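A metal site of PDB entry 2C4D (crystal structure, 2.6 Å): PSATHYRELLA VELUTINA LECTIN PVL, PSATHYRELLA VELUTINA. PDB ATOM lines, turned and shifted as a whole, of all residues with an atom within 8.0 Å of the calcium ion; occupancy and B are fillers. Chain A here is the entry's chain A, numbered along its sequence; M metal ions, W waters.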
ATOM      1  N   ILE A  15       3.924  15.556  -0.692  1.00  0.00           N
ATOM      2  CA  ILE A  15       3.578  16.352  -1.865  1.00  0.00           C
ATOM      3  C   ILE A  15       2.059  16.288  -1.947  1.00  0.00           C
ATOM      4  O   ILE A  15       1.536  15.226  -2.240  1.00  0.00           O
ATOM      5  CB  ILE A  15       4.169  15.743  -3.180  1.00  0.00           C
ATOM      6  CG1 ILE A  15       5.687  15.831  -3.238  1.00  0.00           C
ATOM      7  CG2 ILE A  15       3.599  16.443  -4.428  1.00  0.00           C
ATOM      8  CD1 ILE A  15       6.188  17.200  -3.605  1.00  0.00           C
ATOM      9  N   PRO A  16       1.343  17.383  -1.657  1.00  0.00           N
ATOM     10  CA  PRO A  16       1.749  18.737  -1.236  1.00  0.00           C
ATOM     11  C   PRO A  16       2.178  18.717   0.213  1.00  0.00           C
ATOM     12  O   PRO A  16       1.828  17.810   0.953  1.00  0.00           O
ATOM     13  CB  PRO A  16       0.464  19.569  -1.370  1.00  0.00           C
ATOM     14  CG  PRO A  16      -0.637  18.587  -1.277  1.00  0.00           C
ATOM     15  CD  PRO A  16      -0.131  17.248  -1.752  1.00  0.00           C
ATOM     16  N   GLY A  17       2.973  19.718   0.580  1.00  0.00           N
ATOM     17  CA  GLY A  17       3.568  19.808   1.916  1.00  0.00           C
ATOM     18  C   GLY A  17       4.309  21.099   2.131  1.00  0.00           C
ATOM     19  O   GLY A  17       4.633  21.812   1.197  1.00  0.00           O
ATOM     20  N   VAL A  18       4.524  21.410   3.386  1.00  0.00           N
ATOM     21  CA  VAL A  18       5.353  22.518   3.798  1.00  0.00           C
ATOM     22  C   VAL A  18       6.382  21.928   4.745  1.00  0.00           C
ATOM     23  O   VAL A  18       6.205  21.961   5.966  1.00  0.00           O
ATOM     24  CB  VAL A  18       4.566  23.642   4.524  1.00  0.00           C
ATOM     25  CG1 VAL A  18       3.673  24.306   3.556  1.00  0.00           C
ATOM     26  CG2 VAL A  18       3.748  23.092   5.815  1.00  0.00           C
ATOM     27  N   SER A 288       8.064  15.653  -8.027  1.00  0.00           N
ATOM     28  CA  SER A 288       7.015  16.374  -8.781  1.00  0.00           C
ATOM     29  C   SER A 288       7.122  17.880  -8.660  1.00  0.00           C
ATOM     30  O   SER A 288       6.997  18.409  -7.564  1.00  0.00           O
ATOM     31  CB  SER A 288       5.612  15.997  -8.315  1.00  0.00           C
ATOM     32  OG  SER A 288       5.504  14.606  -8.085  1.00  0.00           O
ATOM     33  N   LEU A 289       7.308  18.565  -9.787  1.00  0.00           N
ATOM     34  CA  LEU A 289       7.352  20.025  -9.825  1.00  0.00           C
ATOM     35  C   LEU A 289       6.154  20.622 -10.511  1.00  0.00           C
ATOM     36  O   LEU A 289       6.165  21.800 -10.797  1.00  0.00           O
ATOM     37  CB  LEU A 289       8.597  20.512 -10.572  1.00  0.00           C
ATOM     38  CG  LEU A 289       9.870  19.668 -10.463  1.00  0.00           C
ATOM     39  CD1 LEU A 289      10.971  20.159 -11.412  1.00  0.00           C
ATOM     40  CD2 LEU A 289      10.372  19.626  -9.014  1.00  0.00           C
ATOM     41  N   VAL A 342      11.906  19.513  -2.537  1.00  0.00           N
ATOM     42  CA  VAL A 342      10.794  19.222  -1.605  1.00  0.00           C
ATOM     43  C   VAL A 342       9.793  20.375  -1.570  1.00  0.00           C
ATOM     44  O   VAL A 342      10.209  21.547  -1.657  1.00  0.00           O
ATOM     45  CB  VAL A 342      11.396  18.959  -0.169  1.00  0.00           C
ATOM     46  CG1 VAL A 342      12.294  20.080   0.271  1.00  0.00           C
ATOM     47  CG2 VAL A 342      10.317  18.782   0.855  1.00  0.00           C
ATOM     48  N   ASP A 343       8.503  20.076  -1.415  1.00  0.00           N
ATOM     49  CA  ASP A 343       7.508  21.162  -1.315  1.00  0.00           C
ATOM     50  C   ASP A 343       7.633  21.895   0.010  1.00  0.00           C
ATOM     51  O   ASP A 343       7.453  21.277   1.065  1.00  0.00           O
ATOM     52  CB  ASP A 343       6.097  20.595  -1.425  1.00  0.00           C
ATOM     53  CG  ASP A 343       5.038  21.634  -1.808  1.00  0.00           C
ATOM     54  OD1 ASP A 343       5.341  22.773  -2.211  1.00  0.00           O
ATOM     55  OD2 ASP A 343       3.854  21.263  -1.735  1.00  0.00           O
ATOM     56  N   LEU A 344       7.925  23.188  -0.057  1.00  0.00           N
ATOM     57  CA  LEU A 344       8.051  24.042   1.113  1.00  0.00           C
ATOM     58  C   LEU A 344       6.913  25.039   1.252  1.00  0.00           C
ATOM     59  O   LEU A 344       6.818  25.751   2.288  1.00  0.00           O
ATOM     60  CB  LEU A 344       9.335  24.867   0.989  1.00  0.00           C
ATOM     61  CG  LEU A 344      10.624  24.043   0.944  1.00  0.00           C
ATOM     62  CD1 LEU A 344      11.791  24.935   0.647  1.00  0.00           C
ATOM     63  CD2 LEU A 344      10.877  23.300   2.254  1.00  0.00           C
ATOM     64  N   THR A 345       6.060  25.128   0.223  1.00  0.00           N
ATOM     65  CA  THR A 345       4.958  26.109   0.151  1.00  0.00           C
ATOM     66  C   THR A 345       3.566  25.473   0.165  1.00  0.00           C
ATOM     67  O   THR A 345       2.566  26.158   0.260  1.00  0.00           O
ATOM     68  CB  THR A 345       5.096  26.933  -1.115  1.00  0.00           C
ATOM     69  OG1 THR A 345       4.810  26.128  -2.283  1.00  0.00           O
ATOM     70  CG2 THR A 345       6.532  27.443  -1.212  1.00  0.00           C
ATOM     71  N   GLY A 346       3.513  24.168   0.061  1.00  0.00           N
ATOM     72  CA  GLY A 346       2.251  23.416   0.144  1.00  0.00           C
ATOM     73  C   GLY A 346       1.406  23.382  -1.113  1.00  0.00           C
ATOM     74  O   GLY A 346       0.274  22.927  -1.041  1.00  0.00           O
ATOM     75  N   ASP A 347       1.914  23.835  -2.259  1.00  0.00           N
ATOM     76  CA  ASP A 347       1.090  23.865  -3.516  1.00  0.00           C
ATOM     77  C   ASP A 347       1.132  22.559  -4.361  1.00  0.00           C
ATOM     78  O   ASP A 347       0.561  22.499  -5.400  1.00  0.00           O
ATOM     79  CB  ASP A 347       1.466  25.031  -4.423  1.00  0.00           C
ATOM     80  CG  ASP A 347       2.861  24.862  -5.041  1.00  0.00           C
ATOM     81  OD1 ASP A 347       3.628  23.984  -4.559  1.00  0.00           O
ATOM     82  OD2 ASP A 347       3.201  25.616  -6.001  1.00  0.00           O
ATOM     83  N   GLY A 348       1.794  21.505  -3.884  1.00  0.00           N
ATOM     84  CA  GLY A 348       2.001  20.303  -4.677  1.00  0.00           C
ATOM     85  C   GLY A 348       3.252  20.306  -5.541  1.00  0.00           C
ATOM     86  O   GLY A 348       3.617  19.293  -6.069  1.00  0.00           O
ATOM     87  N   CYS A 349       3.910  21.448  -5.687  1.00  0.00           N
ATOM     88  CA  CYS A 349       5.040  21.584  -6.587  1.00  0.00           C
ATOM     89  C   CYS A 349       6.330  21.767  -5.811  1.00  0.00           C
ATOM     90  O   CYS A 349       6.478  22.757  -5.031  1.00  0.00           O
ATOM     91  CB  CYS A 349       4.851  22.804  -7.489  1.00  0.00           C
ATOM     92  SG  CYS A 349       3.413  22.702  -8.638  1.00  0.00           S
ATOM     93  N   ALA A 350       7.276  20.861  -6.049  1.00  0.00           N
ATOM     94  CA  ALA A 350       8.437  20.759  -5.181  1.00  0.00           C
ATOM     95  C   ALA A 350       9.337  21.954  -5.333  1.00  0.00           C
ATOM     96  O   ALA A 350       9.419  22.509  -6.428  1.00  0.00           O
ATOM     97  CB  ALA A 350       9.196  19.466  -5.438  1.00  0.00           C
ATOM     98  N   ASP A 351       9.942  22.390  -4.235  1.00  0.00           N
ATOM     99  CA  ASP A 351      10.804  23.542  -4.232  1.00  0.00           C
ATOM    100  C   ASP A 351      12.187  23.059  -3.903  1.00  0.00           C
ATOM    101  O   ASP A 351      12.459  21.878  -3.871  1.00  0.00           O
ATOM    102  CB  ASP A 351      10.327  24.539  -3.213  1.00  0.00           C
ATOM    103  CG  ASP A 351       8.866  24.766  -3.288  1.00  0.00           C
ATOM    104  OD1 ASP A 351       8.394  25.172  -4.347  1.00  0.00           O
ATOM    105  OD2 ASP A 351       8.167  24.514  -2.291  1.00  0.00           O
ATOM    106  N   ILE A 352      13.092  23.979  -3.686  1.00  0.00           N
ATOM    107  CA  ILE A 352      14.507  23.663  -3.509  1.00  0.00           C
ATOM    108  C   ILE A 352      15.051  24.312  -2.260  1.00  0.00           C
ATOM    109  O   ILE A 352      14.861  25.519  -2.051  1.00  0.00           O
ATOM    110  CB  ILE A 352      15.312  24.215  -4.670  1.00  0.00           C
ATOM    111  CG1 ILE A 352      15.091  23.364  -5.916  1.00  0.00           C
ATOM    112  CG2 ILE A 352      16.810  24.291  -4.304  1.00  0.00           C
ATOM    113  CD1 ILE A 352      15.475  24.118  -7.192  1.00  0.00           C
ATOM    114  N   CYS A 363      14.570  28.376  -2.838  1.00  0.00           N
ATOM    115  CA  CYS A 363      14.151  28.782  -4.133  1.00  0.00           C
ATOM    116  C   CYS A 363      12.806  28.141  -4.494  1.00  0.00           C
ATOM    117  O   CYS A 363      12.679  26.926  -4.561  1.00  0.00           O
ATOM    118  CB  CYS A 363      15.237  28.370  -5.114  1.00  0.00           C
ATOM    119  SG  CYS A 363      14.865  29.034  -6.693  1.00  0.00           S
ATOM    120  N   MET A 364      11.790  28.967  -4.725  1.00  0.00           N
ATOM    121  CA  MET A 364      10.417  28.458  -4.784  1.00  0.00           C
ATOM    122  C   MET A 364       9.917  28.200  -6.217  1.00  0.00           C
ATOM    123  O   MET A 364      10.079  29.019  -7.128  1.00  0.00           O
ATOM    124  CB  MET A 364       9.496  29.420  -4.012  1.00  0.00           C
ATOM    125  CG  MET A 364       9.902  29.644  -2.534  1.00  0.00           C
ATOM    126  SD  MET A 364      10.133  28.063  -1.698  1.00  0.00           S
ATOM    127  CE  MET A 364      10.354  28.650  -0.016  1.00  0.00           C
ATOM    128  N   ASN A 365       9.359  27.033  -6.418  1.00  0.00           N
ATOM    129  CA  ASN A 365       8.740  26.670  -7.690  1.00  0.00           C
ATOM    130  C   ASN A 365       7.567  27.628  -7.886  1.00  0.00           C
ATOM    131  O   ASN A 365       6.811  27.860  -6.949  1.00  0.00           O
ATOM    132  CB  ASN A 365       8.316  25.208  -7.570  1.00  0.00           C
ATOM    133  CG  ASN A 365       7.721  24.644  -8.819  1.00  0.00           C
ATOM    134  OD1 ASN A 365       7.197  25.355  -9.635  1.00  0.00           O
ATOM    135  ND2 ASN A 365       7.749  23.342  -8.932  1.00  0.00           N
ATOM    136  N   LYS A 366       7.460  28.246  -9.063  1.00  0.00           N
ATOM    137  CA  LYS A 366       6.338  29.156  -9.383  1.00  0.00           C
ATOM    138  C   LYS A 366       4.986  28.417  -9.504  1.00  0.00           C
ATOM    139  O   LYS A 366       3.938  29.044  -9.540  1.00  0.00           O
ATOM    140  CB  LYS A 366       6.608  29.967 -10.675  1.00  0.00           C
ATOM    141  CG  LYS A 366       7.377  31.277 -10.418  1.00  0.00           C
ATOM    142  CD  LYS A 366       8.071  31.873 -11.698  1.00  0.00           C
ATOM    143  CE  LYS A 366       8.615  33.320 -11.446  1.00  0.00           C
ATOM    144  NZ  LYS A 366       9.634  33.757 -12.482  1.00  0.00           N
ATOM    145  N   GLY A 367       4.995  27.091  -9.552  1.00  0.00           N
ATOM    146  CA  GLY A 367       3.768  26.323  -9.681  1.00  0.00           C
ATOM    147  C   GLY A 367       3.739  25.564 -10.992  1.00  0.00           C
ATOM    148  O   GLY A 367       2.969  24.614 -11.137  1.00  0.00           O
ATOM    149  N   PHE A 371      10.983  28.687 -11.625  1.00  0.00           N
ATOM    150  CA  PHE A 371      11.405  28.962 -10.280  1.00  0.00           C
ATOM    151  C   PHE A 371      11.616  30.436 -10.038  1.00  0.00           C
ATOM    152  O   PHE A 371      11.812  31.186 -10.970  1.00  0.00           O
ATOM    153  CB  PHE A 371      12.658  28.154  -9.976  1.00  0.00           C
ATOM    154  CG  PHE A 371      12.353  26.715  -9.607  1.00  0.00           C
ATOM    155  CD1 PHE A 371      12.276  26.329  -8.252  1.00  0.00           C
ATOM    156  CD2 PHE A 371      12.132  25.765 -10.585  1.00  0.00           C
ATOM    157  CE1 PHE A 371      11.989  25.036  -7.881  1.00  0.00           C
ATOM    158  CE2 PHE A 371      11.848  24.434 -10.228  1.00  0.00           C
ATOM    159  CZ  PHE A 371      11.768  24.072  -8.876  1.00  0.00           C
HETATM  160 CA    CA M   1       6.106  24.509  -3.588  1.00  0.00          CA
HETATM  161  O   HOH W   1       5.712  26.068  -5.362  1.00  0.00           O
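The backbone NH (N) of Asp 351 is in hydrogen-bond range of the backbone carbonyl oxygen (O) of Val 342. The backbone carbonyl oxygen (O) of Gly 367 lies within hydrogen-bond range of the side-chain sulfur (SG) of Cys 349 (3.2 Å). The side-chain carboxylate of Asp 351 sits close to the backbone NH of Leu 344 (2.6 Å). OD2 of Asp 343 lies close to N of Gly 346, 3.4 Å away. The side-chain carboxylate (OD2) of Asp 343 lies within hydrogen-bond range of the backbone NH (N) of Gly 348. SG of Cys 349 sits at hydrogen-bond distance from O of Leu 289, at 3.6 Å. The side-chain carboxylate of Asp 343 lies within hydrogen-bond range of the backbone NH of Gly 17 (2.9 Å). The side-chain carboxylate (OD1) of Asp 351 lies close to the backbone NH (N) of Asn 365.
The calcium ion is bound by O of Cys 349. OD1 of Asp 343 is bound to the calcium ion (2.3 Å). Water W1 is bound to the calcium ion (2.4 Å). The calcium ion is bound by OD2 of Asp 351 (2.4 Å). OG1 of Thr 345 binds the calcium ion, at 2.5 Å. OD1 of Asp 351 binds the calcium ion (2.5 Å). The calcium ion is bound by OD1 of Asp 347. The calcium ion has seven donor atoms within binding distance.
Water W1 bridges OD2 of Asp 347 (2.6 Å) and O of Asn 365 (2.6 Å).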
